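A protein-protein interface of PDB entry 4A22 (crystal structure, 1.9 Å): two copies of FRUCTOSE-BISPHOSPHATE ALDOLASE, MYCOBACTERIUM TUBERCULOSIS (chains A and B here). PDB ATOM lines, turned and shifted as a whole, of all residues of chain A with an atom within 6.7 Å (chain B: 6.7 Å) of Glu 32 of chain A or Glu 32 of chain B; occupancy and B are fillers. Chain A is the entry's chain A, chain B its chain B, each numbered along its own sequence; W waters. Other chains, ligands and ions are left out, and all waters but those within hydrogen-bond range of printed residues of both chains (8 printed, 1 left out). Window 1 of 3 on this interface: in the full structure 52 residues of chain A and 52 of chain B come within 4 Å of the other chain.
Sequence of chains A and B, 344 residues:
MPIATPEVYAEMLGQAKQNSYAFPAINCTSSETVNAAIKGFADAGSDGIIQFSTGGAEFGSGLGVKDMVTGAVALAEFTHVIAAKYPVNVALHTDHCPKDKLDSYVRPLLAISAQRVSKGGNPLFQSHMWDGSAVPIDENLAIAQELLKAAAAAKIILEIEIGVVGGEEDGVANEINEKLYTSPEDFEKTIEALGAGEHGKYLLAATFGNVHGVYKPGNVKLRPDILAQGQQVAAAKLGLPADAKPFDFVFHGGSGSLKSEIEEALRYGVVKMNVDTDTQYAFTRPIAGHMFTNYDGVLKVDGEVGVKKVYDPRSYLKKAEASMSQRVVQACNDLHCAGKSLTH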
ATOM      1  N   THR A  29      14.759  22.698 -28.630  1.00  0.00           N
ATOM      2  CA  THR A  29      14.194  22.813 -27.289  1.00  0.00           C
ATOM      3  C   THR A  29      15.163  22.913 -26.096  1.00  0.00           C
ATOM      4  O   THR A  29      14.723  22.946 -24.941  1.00  0.00           O
ATOM      5  CB  THR A  29      13.271  21.640 -27.094  1.00  0.00           C
ATOM      6  OG1 THR A  29      14.047  20.449 -27.275  1.00  0.00           O
ATOM      7  CG2 THR A  29      12.161  21.690 -28.159  1.00  0.00           C
ATOM      8  N   SER A  30      16.465  22.905 -26.358  1.00  0.00           N
ATOM      9  CA  SER A  30      17.444  22.632 -25.316  1.00  0.00           C
ATOM     10  C   SER A  30      18.825  22.845 -25.862  1.00  0.00           C
ATOM     11  O   SER A  30      19.024  22.955 -27.084  1.00  0.00           O
ATOM     12  CB  SER A  30      17.386  21.161 -24.886  1.00  0.00           C
ATOM     13  OG  SER A  30      17.829  20.334 -25.962  1.00  0.00           O
ATOM     14  N   SER A  31      19.785  22.858 -24.947  1.00  0.00           N
ATOM     15  CA  SER A  31      21.183  22.983 -25.320  1.00  0.00           C
ATOM     16  C   SER A  31      21.613  21.858 -26.271  1.00  0.00           C
ATOM     17  O   SER A  31      22.328  22.115 -27.230  1.00  0.00           O
ATOM     18  CB  SER A  31      22.058  22.994 -24.062  1.00  0.00           C
ATOM     19  OG  SER A  31      21.851  21.823 -23.289  1.00  0.00           O
ATOM     20  N   GLU A  32      21.190  20.616 -26.011  1.00  0.00           N
ATOM     21  CA  GLU A  32      21.602  19.494 -26.860  1.00  0.00           C
ATOM     22  C   GLU A  32      21.088  19.609 -28.313  1.00  0.00           C
ATOM     23  O   GLU A  32      21.826  19.320 -29.252  1.00  0.00           O
ATOM     24  CB  GLU A  32      21.151  18.150 -26.273  1.00  0.00           C
ATOM     25  CG  GLU A  32      21.663  17.883 -24.867  1.00  0.00           C
ATOM     26  CD  GLU A  32      20.657  18.288 -23.799  1.00  0.00           C
ATOM     27  OE1 GLU A  32      19.910  19.269 -24.013  1.00  0.00           O
ATOM     28  OE2 GLU A  32      20.606  17.618 -22.745  1.00  0.00           O
ATOM     29  N   THR A  33      19.836  20.017 -28.496  1.00  0.00           N
ATOM     30  CA  THR A  33      19.272  20.101 -29.836  1.00  0.00           C
ATOM     31  C   THR A  33      19.815  21.308 -30.600  1.00  0.00           C
ATOM     32  O   THR A  33      20.014  21.226 -31.798  1.00  0.00           O
ATOM     33  CB  THR A  33      17.719  20.107 -29.837  1.00  0.00           C
ATOM     34  OG1 THR A  33      17.226  21.111 -28.946  1.00  0.00           O
ATOM     35  CG2 THR A  33      17.186  18.742 -29.409  1.00  0.00           C
ATOM     36  N   VAL A  34      20.078  22.415 -29.899  1.00  0.00           N
ATOM     37  CA  VAL A  34      20.725  23.569 -30.516  1.00  0.00           C
ATOM     38  C   VAL A  34      22.122  23.159 -30.978  1.00  0.00           C
ATOM     39  O   VAL A  34      22.520  23.472 -32.093  1.00  0.00           O
ATOM     40  CB  VAL A  34      20.817  24.795 -29.551  1.00  0.00           C
ATOM     41  CG1 VAL A  34      21.851  25.807 -30.054  1.00  0.00           C
ATOM     42  CG2 VAL A  34      19.459  25.492 -29.422  1.00  0.00           C
ATOM     43  N   ASN A  35      22.880  22.473 -30.113  1.00  0.00           N
ATOM     44  CA  ASN A  35      24.187  21.979 -30.513  1.00  0.00           C
ATOM     45  C   ASN A  35      24.105  21.059 -31.724  1.00  0.00           C
ATOM     46  O   ASN A  35      24.909  21.165 -32.627  1.00  0.00           O
ATOM     47  CB  ASN A  35      24.876  21.262 -29.355  1.00  0.00           C
ATOM     48  CG  ASN A  35      25.479  22.235 -28.395  1.00  0.00           C
ATOM     49  OD1 ASN A  35      25.849  23.316 -28.810  1.00  0.00           O
ATOM     50  ND2 ASN A  35      25.550  21.885 -27.110  1.00  0.00           N
ATOM     51  N   ALA A  36      23.132  20.160 -31.732  1.00  0.00           N
ATOM     52  CA  ALA A  36      22.962  19.225 -32.853  1.00  0.00           C
ATOM     53  C   ALA A  36      22.687  19.952 -34.176  1.00  0.00           C
ATOM     54  O   ALA A  36      23.260  19.623 -35.214  1.00  0.00           O
ATOM     55  CB  ALA A  36      21.809  18.254 -32.556  1.00  0.00           C
ATOM     56  N   ALA A  37      21.799  20.939 -34.126  1.00  0.00           N
ATOM     57  CA  ALA A  37      21.402  21.682 -35.305  1.00  0.00           C
ATOM     58  C   ALA A  37      22.586  22.460 -35.856  1.00  0.00           C
ATOM     59  O   ALA A  37      22.847  22.415 -37.051  1.00  0.00           O
ATOM     60  CB  ALA A  37      20.211  22.636 -34.992  1.00  0.00           C
ATOM     61  N   PHE A  59       9.259  24.882 -22.621  1.00  0.00           N
ATOM     62  CA  PHE A  59      10.031  23.726 -22.178  1.00  0.00           C
ATOM     63  C   PHE A  59      11.437  24.130 -21.742  1.00  0.00           C
ATOM     64  O   PHE A  59      11.936  23.663 -20.714  1.00  0.00           O
ATOM     65  CB  PHE A  59      10.162  22.666 -23.297  1.00  0.00           C
ATOM     66  CG  PHE A  59      11.074  21.511 -22.925  1.00  0.00           C
ATOM     67  CD1 PHE A  59      10.628  20.488 -22.084  1.00  0.00           C
ATOM     68  CD2 PHE A  59      12.378  21.455 -23.405  1.00  0.00           C
ATOM     69  CE1 PHE A  59      11.472  19.448 -21.725  1.00  0.00           C
ATOM     70  CE2 PHE A  59      13.220  20.405 -23.066  1.00  0.00           C
ATOM     71  CZ  PHE A  59      12.778  19.409 -22.218  1.00  0.00           C
ATOM     72  N   GLY A  60      12.071  24.971 -22.549  1.00  0.00           N
ATOM     73  CA  GLY A  60      13.422  25.460 -22.290  1.00  0.00           C
ATOM     74  C   GLY A  60      13.542  26.308 -21.040  1.00  0.00           C
ATOM     75  O   GLY A  60      14.630  26.418 -20.467  1.00  0.00           O
ATOM     76  N   PHE A  78      22.346  31.179 -24.793  1.00  0.00           N
ATOM     77  CA  PHE A  78      23.164  29.985 -24.980  1.00  0.00           C
ATOM     78  C   PHE A  78      23.652  29.925 -26.424  1.00  0.00           C
ATOM     79  O   PHE A  78      24.840  29.728 -26.683  1.00  0.00           O
ATOM     80  CB  PHE A  78      22.365  28.711 -24.669  1.00  0.00           C
ATOM     81  CG  PHE A  78      23.122  27.436 -24.927  1.00  0.00           C
ATOM     82  CD1 PHE A  78      23.931  26.875 -23.947  1.00  0.00           C
ATOM     83  CD2 PHE A  78      23.007  26.784 -26.145  1.00  0.00           C
ATOM     84  CE1 PHE A  78      24.626  25.685 -24.202  1.00  0.00           C
ATOM     85  CE2 PHE A  78      23.686  25.603 -26.393  1.00  0.00           C
ATOM     86  CZ  PHE A  78      24.503  25.055 -25.417  1.00  0.00           C
ATOM     87  N   PHE A 283      16.666  12.401 -33.051  1.00  0.00           N
ATOM     88  CA  PHE A 283      17.244  12.641 -31.740  1.00  0.00           C
ATOM     89  C   PHE A 283      16.956  11.461 -30.809  1.00  0.00           C
ATOM     90  O   PHE A 283      17.829  10.966 -30.128  1.00  0.00           O
ATOM     91  CB  PHE A 283      16.629  13.891 -31.129  1.00  0.00           C
ATOM     92  CG  PHE A 283      17.346  14.375 -29.890  1.00  0.00           C
ATOM     93  CD1 PHE A 283      18.464  15.187 -29.997  1.00  0.00           C
ATOM     94  CD2 PHE A 283      16.886  14.036 -28.633  1.00  0.00           C
ATOM     95  CE1 PHE A 283      19.110  15.637 -28.861  1.00  0.00           C
ATOM     96  CE2 PHE A 283      17.530  14.472 -27.505  1.00  0.00           C
ATOM     97  CZ  PHE A 283      18.634  15.279 -27.609  1.00  0.00           C
ATOM     98  N   PRO A 313      23.777  10.642 -18.510  1.00  0.00           N
ATOM     99  CA  PRO A 313      22.964  11.170 -19.620  1.00  0.00           C
ATOM    100  C   PRO A 313      23.791  11.540 -20.844  1.00  0.00           C
ATOM    101  O   PRO A 313      23.282  11.487 -21.952  1.00  0.00           O
ATOM    102  CB  PRO A 313      22.327  12.434 -19.036  1.00  0.00           C
ATOM    103  CG  PRO A 313      22.279  12.172 -17.553  1.00  0.00           C
ATOM    104  CD  PRO A 313      23.469  11.311 -17.232  1.00  0.00           C
ATOM    105  N   LEU A 317      22.882  11.048 -24.797  1.00  0.00           N
ATOM    106  CA  LEU A 317      22.613  12.359 -25.412  1.00  0.00           C
ATOM    107  C   LEU A 317      23.636  12.720 -26.505  1.00  0.00           C
ATOM    108  O   LEU A 317      23.286  13.396 -27.466  1.00  0.00           O
ATOM    109  CB  LEU A 317      22.520  13.491 -24.368  1.00  0.00           C
ATOM    110  CG  LEU A 317      21.362  13.329 -23.372  1.00  0.00           C
ATOM    111  CD1 LEU A 317      21.428  14.343 -22.236  1.00  0.00           C
ATOM    112  CD2 LEU A 317      20.033  13.411 -24.113  1.00  0.00           C
ATOM    113  N   LYS A 318      24.882  12.277 -26.379  1.00  0.00           N
ATOM    114  CA  LYS A 318      25.853  12.499 -27.467  1.00  0.00           C
ATOM    115  C   LYS A 318      25.404  11.755 -28.722  1.00  0.00           C
ATOM    116  O   LYS A 318      25.580  12.235 -29.839  1.00  0.00           O
ATOM    117  CB  LYS A 318      27.250  12.015 -27.081  1.00  0.00           C
ATOM    118  CG  LYS A 318      28.001  12.969 -26.161  1.00  0.00           C
ATOM    119  CD  LYS A 318      29.421  12.470 -25.855  1.00  0.00           C
ATOM    120  CE  LYS A 318      29.414  11.187 -25.042  1.00  0.00           C
ATOM    121  NZ  LYS A 318      30.782  10.613 -24.906  1.00  0.00           N
ATOM    122  N   ALA A 320      22.247  11.000 -29.474  1.00  0.00           N
ATOM    123  CA  ALA A 320      21.082  11.745 -29.960  1.00  0.00           C
ATOM    124  C   ALA A 320      21.537  12.965 -30.738  1.00  0.00           C
ATOM    125  O   ALA A 320      21.035  13.269 -31.807  1.00  0.00           O
ATOM    126  CB  ALA A 320      20.184  12.186 -28.782  1.00  0.00           C
ATOM    127  N   GLU A 321      22.524  13.657 -30.197  1.00  0.00           N
ATOM    128  CA  GLU A 321      23.024  14.870 -30.838  1.00  0.00           C
ATOM    129  C   GLU A 321      23.569  14.564 -32.235  1.00  0.00           C
ATOM    130  O   GLU A 321      23.194  15.231 -33.223  1.00  0.00           O
ATOM    131  CB  GLU A 321      24.130  15.490 -29.967  1.00  0.00           C
ATOM    132  CG  GLU A 321      24.524  16.874 -30.434  1.00  0.00           C
ATOM    133  CD  GLU A 321      25.734  17.439 -29.708  1.00  0.00           C
ATOM    134  OE1 GLU A 321      25.861  17.212 -28.481  1.00  0.00           O
ATOM    135  OE2 GLU A 321      26.551  18.114 -30.377  1.00  0.00           O
ATOM    136  N   MET A 324      20.807  13.575 -34.668  1.00  0.00           N
ATOM    137  CA  MET A 324      20.049  14.732 -35.113  1.00  0.00           C
ATOM    138  C   MET A 324      20.876  15.588 -36.094  1.00  0.00           C
ATOM    139  O   MET A 324      20.339  16.053 -37.090  1.00  0.00           O
ATOM    140  CB  MET A 324      19.579  15.582 -33.930  1.00  0.00           C
ATOM    141  CG  MET A 324      18.756  16.790 -34.332  1.00  0.00           C
ATOM    142  SD  MET A 324      18.015  17.572 -32.896  1.00  0.00           S
ATOM    143  CE  MET A 324      17.664  19.217 -33.574  1.00  0.00           C
ATOM    144  N   THR B  29      25.005  19.173 -17.050  1.00  0.00           N
ATOM    145  CA  THR B  29      25.567  19.157 -18.400  1.00  0.00           C
ATOM    146  C   THR B  29      24.762  19.863 -19.506  1.00  0.00           C
ATOM    147  O   THR B  29      25.144  19.822 -20.669  1.00  0.00           O
ATOM    148  CB  THR B  29      25.770  17.699 -18.819  1.00  0.00           C
ATOM    149  OG1 THR B  29      24.513  17.019 -18.712  1.00  0.00           O
ATOM    150  CG2 THR B  29      26.802  17.031 -17.889  1.00  0.00           C
ATOM    151  N   SER B  30      23.609  20.421 -19.178  1.00  0.00           N
ATOM    152  CA  SER B  30      22.697  20.856 -20.228  1.00  0.00           C
ATOM    153  C   SER B  30      21.617  21.738 -19.668  1.00  0.00           C
ATOM    154  O   SER B  30      21.494  21.894 -18.446  1.00  0.00           O
ATOM    155  CB  SER B  30      22.014  19.625 -20.846  1.00  0.00           C
ATOM    156  OG  SER B  30      21.256  18.939 -19.853  1.00  0.00           O
ATOM    157  N   SER B  31      20.797  22.271 -20.565  1.00  0.00           N
ATOM    158  CA  SER B  31      19.687  23.112 -20.173  1.00  0.00           C
ATOM    159  C   SER B  31      18.729  22.313 -19.307  1.00  0.00           C
ATOM    160  O   SER B  31      18.296  22.796 -18.263  1.00  0.00           O
ATOM    161  CB  SER B  31      18.970  23.689 -21.409  1.00  0.00           C
ATOM    162  OG  SER B  31      18.701  22.702 -22.375  1.00  0.00           O
ATOM    163  N   GLU B  32      18.414  21.078 -19.707  1.00  0.00           N
ATOM    164  CA  GLU B  32      17.449  20.295 -18.936  1.00  0.00           C
ATOM    165  C   GLU B  32      17.912  20.009 -17.498  1.00  0.00           C
ATOM    166  O   GLU B  32      17.109  20.090 -16.568  1.00  0.00           O
ATOM    167  CB  GLU B  32      17.127  18.958 -19.621  1.00  0.00           C
ATOM    168  CG  GLU B  32      16.488  19.127 -20.979  1.00  0.00           C
ATOM    169  CD  GLU B  32      17.501  19.060 -22.109  1.00  0.00           C
ATOM    170  OE1 GLU B  32      18.713  19.264 -21.855  1.00  0.00           O
ATOM    171  OE2 GLU B  32      17.079  18.787 -23.254  1.00  0.00           O
ATOM    172  N   THR B  33      19.177  19.640 -17.325  1.00  0.00           N
ATOM    173  CA  THR B  33      19.690  19.329 -15.982  1.00  0.00           C
ATOM    174  C   THR B  33      19.855  20.586 -15.126  1.00  0.00           C
ATOM    175  O   THR B  33      19.648  20.550 -13.923  1.00  0.00           O
ATOM    176  CB  THR B  33      21.022  18.560 -16.030  1.00  0.00           C
ATOM    177  OG1 THR B  33      21.953  19.240 -16.885  1.00  0.00           O
ATOM    178  CG2 THR B  33      20.802  17.143 -16.574  1.00  0.00           C
ATOM    179  N   VAL B  34      20.251  21.699 -15.732  1.00  0.00           N
ATOM    180  CA  VAL B  34      20.325  22.960 -14.982  1.00  0.00           C
ATOM    181  C   VAL B  34      18.910  23.315 -14.501  1.00  0.00           C
ATOM    182  O   VAL B  34      18.705  23.657 -13.358  1.00  0.00           O
ATOM    183  CB  VAL B  34      20.844  24.119 -15.860  1.00  0.00           C
ATOM    184  CG1 VAL B  34      20.560  25.477 -15.198  1.00  0.00           C
ATOM    185  CG2 VAL B  34      22.315  23.944 -16.153  1.00  0.00           C
ATOM    186  N   ASN B  35      17.923  23.218 -15.393  1.00  0.00           N
ATOM    187  CA  ASN B  35      16.539  23.473 -14.999  1.00  0.00           C
ATOM    188  C   ASN B  35      16.060  22.567 -13.871  1.00  0.00           C
ATOM    189  O   ASN B  35      15.358  23.022 -12.980  1.00  0.00           O
ATOM    190  CB  ASN B  35      15.613  23.327 -16.199  1.00  0.00           C
ATOM    191  CG  ASN B  35      15.571  24.590 -17.062  1.00  0.00           C
ATOM    192  OD1 ASN B  35      15.903  25.671 -16.599  1.00  0.00           O
ATOM    193  ND2 ASN B  35      15.148  24.448 -18.321  1.00  0.00           N
ATOM    194  N   ALA B  36      16.423  21.286 -13.932  1.00  0.00           N
ATOM    195  CA  ALA B  36      16.002  20.321 -12.912  1.00  0.00           C
ATOM    196  C   ALA B  36      16.605  20.693 -11.572  1.00  0.00           C
ATOM    197  O   ALA B  36      15.946  20.640 -10.537  1.00  0.00           O
ATOM    198  CB  ALA B  36      16.441  18.903 -13.307  1.00  0.00           C
ATOM    199  N   ALA B  37      17.876  21.067 -11.613  1.00  0.00           N
ATOM    200  CA  ALA B  37      18.624  21.356 -10.406  1.00  0.00           C
ATOM    201  C   ALA B  37      18.019  22.571  -9.707  1.00  0.00           C
ATOM    202  O   ALA B  37      17.733  22.537  -8.512  1.00  0.00           O
ATOM    203  CB  ALA B  37      20.104  21.578 -10.740  1.00  0.00           C
ATOM    204  N   PHE B  59      30.895  18.628 -23.088  1.00  0.00           N
ATOM    205  CA  PHE B  59      29.617  18.132 -23.611  1.00  0.00           C
ATOM    206  C   PHE B  59      28.701  19.300 -23.962  1.00  0.00           C
ATOM    207  O   PHE B  59      28.065  19.348 -25.028  1.00  0.00           O
ATOM    208  CB  PHE B  59      28.926  17.255 -22.572  1.00  0.00           C
ATOM    209  CG  PHE B  59      27.535  16.836 -22.980  1.00  0.00           C
ATOM    210  CD1 PHE B  59      27.346  15.799 -23.897  1.00  0.00           C
ATOM    211  CD2 PHE B  59      26.423  17.509 -22.492  1.00  0.00           C
ATOM    212  CE1 PHE B  59      26.066  15.430 -24.290  1.00  0.00           C
ATOM    213  CE2 PHE B  59      25.131  17.140 -22.876  1.00  0.00           C
ATOM    214  CZ  PHE B  59      24.956  16.103 -23.778  1.00  0.00           C
ATOM    215  N   GLY B  60      28.632  20.242 -23.037  1.00  0.00           N
ATOM    216  CA  GLY B  60      27.818  21.435 -23.188  1.00  0.00           C
ATOM    217  C   GLY B  60      28.186  22.270 -24.404  1.00  0.00           C
ATOM    218  O   GLY B  60      27.321  22.947 -24.933  1.00  0.00           O
ATOM    219  N   PHE B  78      23.026  30.706 -20.084  1.00  0.00           N
ATOM    220  CA  PHE B  78      21.688  30.120 -19.970  1.00  0.00           C
ATOM    221  C   PHE B  78      21.183  30.227 -18.524  1.00  0.00           C
ATOM    222  O   PHE B  78      20.045  30.640 -18.263  1.00  0.00           O
ATOM    223  CB  PHE B  78      21.733  28.647 -20.352  1.00  0.00           C
ATOM    224  CG  PHE B  78      20.415  27.947 -20.177  1.00  0.00           C
ATOM    225  CD1 PHE B  78      19.472  27.966 -21.194  1.00  0.00           C
ATOM    226  CD2 PHE B  78      20.112  27.282 -18.991  1.00  0.00           C
ATOM    227  CE1 PHE B  78      18.252  27.350 -21.026  1.00  0.00           C
ATOM    228  CE2 PHE B  78      18.891  26.664 -18.812  1.00  0.00           C
ATOM    229  CZ  PHE B  78      17.959  26.684 -19.850  1.00  0.00           C
ATOM    230  N   PHE B 283      17.762  11.139 -13.363  1.00  0.00           N
ATOM    231  CA  PHE B 283      17.417  11.716 -14.670  1.00  0.00           C
ATOM    232  C   PHE B 283      17.112  10.622 -15.687  1.00  0.00           C
ATOM    233  O   PHE B 283      16.110  10.667 -16.406  1.00  0.00           O
ATOM    234  CB  PHE B 283      18.573  12.574 -15.165  1.00  0.00           C
ATOM    235  CG  PHE B 283      18.259  13.376 -16.401  1.00  0.00           C
ATOM    236  CD1 PHE B 283      17.689  14.635 -16.301  1.00  0.00           C
ATOM    237  CD2 PHE B 283      18.557  12.877 -17.653  1.00  0.00           C
ATOM    238  CE1 PHE B 283      17.421  15.390 -17.434  1.00  0.00           C
ATOM    239  CE2 PHE B 283      18.301  13.625 -18.782  1.00  0.00           C
ATOM    240  CZ  PHE B 283      17.721  14.885 -18.674  1.00  0.00           C
ATOM    241  N   PRO B 313      11.182  14.655 -27.917  1.00  0.00           N
ATOM    242  CA  PRO B 313      12.075  14.596 -26.753  1.00  0.00           C
ATOM    243  C   PRO B 313      11.488  15.211 -25.488  1.00  0.00           C
ATOM    244  O   PRO B 313      11.814  14.744 -24.408  1.00  0.00           O
ATOM    245  CB  PRO B 313      13.303  15.389 -27.214  1.00  0.00           C
ATOM    246  CG  PRO B 313      13.345  15.146 -28.691  1.00  0.00           C
ATOM    247  CD  PRO B 313      11.887  15.111 -29.127  1.00  0.00           C
ATOM    248  N   LEU B 317      11.865  13.981 -21.621  1.00  0.00           N
ATOM    249  CA  LEU B 317      12.787  14.867 -20.914  1.00  0.00           C
ATOM    250  C   LEU B 317      12.117  15.605 -19.758  1.00  0.00           C
ATOM    251  O   LEU B 317      12.789  15.985 -18.791  1.00  0.00           O
ATOM    252  CB  LEU B 317      13.457  15.847 -21.874  1.00  0.00           C
ATOM    253  CG  LEU B 317      14.464  15.181 -22.820  1.00  0.00           C
ATOM    254  CD1 LEU B 317      15.062  16.192 -23.828  1.00  0.00           C
ATOM    255  CD2 LEU B 317      15.570  14.503 -22.039  1.00  0.00           C
ATOM    256  N   LYS B 318      10.809  15.842 -19.860  1.00  0.00           N
ATOM    257  CA  LYS B 318      10.071  16.459 -18.761  1.00  0.00           C
ATOM    258  C   LYS B 318      10.005  15.498 -17.598  1.00  0.00           C
ATOM    259  O   LYS B 318      10.057  15.930 -16.458  1.00  0.00           O
ATOM    260  CB  LYS B 318       8.638  16.789 -19.152  1.00  0.00           C
ATOM    261  CG  LYS B 318       8.419  18.133 -19.812  1.00  0.00           C
ATOM    262  CD  LYS B 318       6.908  18.319 -19.941  1.00  0.00           C
ATOM    263  CE  LYS B 318       6.496  19.349 -20.958  1.00  0.00           C
ATOM    264  NZ  LYS B 318       5.143  18.982 -21.467  1.00  0.00           N
ATOM    265  N   ALA B 320      12.291  13.148 -16.991  1.00  0.00           N
ATOM    266  CA  ALA B 320      13.668  13.121 -16.498  1.00  0.00           C
ATOM    267  C   ALA B 320      13.942  14.299 -15.568  1.00  0.00           C
ATOM    268  O   ALA B 320      14.560  14.139 -14.516  1.00  0.00           O
ATOM    269  CB  ALA B 320      14.634  13.153 -17.654  1.00  0.00           C
ATOM    270  N   GLU B 321      13.507  15.483 -15.982  1.00  0.00           N
ATOM    271  CA  GLU B 321      13.775  16.717 -15.240  1.00  0.00           C
ATOM    272  C   GLU B 321      13.056  16.686 -13.893  1.00  0.00           C
ATOM    273  O   GLU B 321      13.629  17.051 -12.862  1.00  0.00           O
ATOM    274  CB  GLU B 321      13.334  17.937 -16.072  1.00  0.00           C
ATOM    275  CG  GLU B 321      13.642  19.286 -15.454  1.00  0.00           C
ATOM    276  CD  GLU B 321      12.764  20.427 -16.002  1.00  0.00           C
ATOM    277  OE1 GLU B 321      12.517  20.468 -17.227  1.00  0.00           O
ATOM    278  OE2 GLU B 321      12.329  21.289 -15.199  1.00  0.00           O
ATOM    279  N   MET B 324      14.830  14.224 -11.580  1.00  0.00           N
ATOM    280  CA  MET B 324      16.055  14.819 -11.063  1.00  0.00           C
ATOM    281  C   MET B 324      15.749  15.862  -9.996  1.00  0.00           C
ATOM    282  O   MET B 324      16.412  15.895  -8.955  1.00  0.00           O
ATOM    283  CB  MET B 324      16.864  15.443 -12.195  1.00  0.00           C
ATOM    284  CG  MET B 324      18.190  15.970 -11.723  1.00  0.00           C
ATOM    285  SD  MET B 324      19.268  16.327 -13.094  1.00  0.00           S
ATOM    286  CE  MET B 324      20.386  17.506 -12.291  1.00  0.00           C
ATOM    287  N   SER B 325      14.747  16.713 -10.234  1.00  0.00           N
ATOM    288  CA  SER B 325      14.411  17.738  -9.247  1.00  0.00           C
ATOM    289  C   SER B 325      14.013  17.087  -7.919  1.00  0.00           C
ATOM    290  O   SER B 325      14.399  17.561  -6.856  1.00  0.00           O
ATOM    291  CB  SER B 325      13.310  18.664  -9.734  1.00  0.00           C
ATOM    292  OG  SER B 325      13.725  19.362 -10.891  1.00  0.00           O
HETATM  293  O   HOH W   1      15.368  18.455 -26.130  1.00  0.00           O
HETATM  294  O   HOH W   2      23.978  20.377 -23.421  1.00  0.00           O
HETATM  295  O   HOH W   3      15.968  22.511 -22.397  1.00  0.00           O
HETATM  296  O   HOH W   4      17.797  17.749 -25.558  1.00  0.00           O
HETATM  297  O   HOH W   5      10.888  21.679 -18.993  1.00  0.00           O
HETATM  298  O   HOH W   6      25.201  19.604 -25.699  1.00  0.00           O
HETATM  299  O   HOH W   7      28.049  17.222 -26.851  1.00  0.00           O
HETATM  300  O   HOH W   8      14.373  22.225 -20.004  1.00  0.00           O
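The side-chain hydroxyl (OG1) of Thr 33 of chain A is in hydrogen-bond range of the side-chain hydroxyl (OG) of Ser 30 of chain A (3.1 Å). OE1 of Glu 32 of chain B is in hydrogen-bond range of OG of Ser 30 of chain B (3.3 Å).
Among the printed residues, merely in contact across the chains: Ser 30 of chain A with Ser 31 of chain B, Ser 31 of chain A with Ser 30 of chain B, Gly 60 of chain A with Phe 78 of chain B, Phe 78 of chain A with Gly 60 of chain B, Leu 317 of chain A with Phe 59 of chain B, Phe 59 of chain A with Leu 317 of chain B, Lys 318 of chain A with Phe 59 of chain B, Phe 283 of chain A with Pro 313 of chain B, Pro 313 of chain A with Phe 283 of chain B, Phe 59 of chain A with Lys 318 of chain B, Glu 32 of chain A with Phe 59 of chain B, Phe 59 of chain A with Glu 32 of chain B and Glu 32 of chain A with Ser 31 of chain B.
Printed residues of chain A that touch a printed residue of chain B: Ser 30, Ser 31, Glu 32, Asn 35, Phe 59, Gly 60, Phe 78, Phe 283, Pro 313, Leu 317 and Lys 318. Of the 20 printed residues of chain B, 11 touch a printed residue of chain A. Among the printed residues, no Asp or Glu carboxylate lies within 4 Å of a Lys or Arg side-chain nitrogen of the other chain.
The backbone carbonyl oxygen (O) of Gly 60 of chain A sits at hydrogen-bond distance from the side-chain amide nitrogen (ND2) of Asn 35 of chain B (3.0 Å). The backbone NH of Ser 31 of chain A lies within hydrogen-bond range of the side-chain hydroxyl of Ser 31 of chain B, at 2.8 Å. The side-chain carboxylate (OE2) of Glu 32 of chain A lies close to the side-chain hydroxyl (OG) of Ser 30 of chain B. The side-chain carboxylate (OE1) of Glu 32 of chain A sits close to the side-chain carboxylate (OE1) of Glu 32 of chain B, at 2.5 Å. ND2 of Asn 35 of chain A sits at hydrogen-bond distance from O of Gly 60 of chain B (3.0 Å). OG of Ser 30 of chain A lies close to OE2 of Glu 32 of chain B.
Water W2 lies within hydrogen-bond range of OG of Ser 31 of chain A (2.6 Å) and O of Thr 29 of chain B (3.0 Å). Water W6 bridges ND2 of Asn 35 of chain A (2.7 Å) and O of Phe 59 of chain B (3.0 Å). Water W7 lies within hydrogen-bond range of OE1 of Glu 321 of chain A (2.7 Å) and O of Phe 59 of chain B (2.8 Å).
Of the printed residues of chain B, Glu 32 of chain A touches Ser 30, Ser 31, Glu 32 and Phe 59. Printed residues of chain B within 4 Å of Phe 78 of chain A: Gly 60. Printed residues of chain B within 4 Å of Phe 283 of chain A: Pro 313 (3.7 Å). The nearest printed residue of chain B that does not touch Glu 32 of chain A is Thr 29 of chain B (5.5 Å). The nearest printed residue of chain B that does not touch Pro 313 of chain A is Thr 29 of chain B (5.1 Å).
Ser 30 of chain A touches Ser 31 of chain B, and with the chains exchanged Ser 31 of chain A touches Ser 30 of chain B. Phe 283 of chain A touches Pro 313 of chain B, and with the chains exchanged Pro 313 of chain A touches Phe 283 of chain B.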
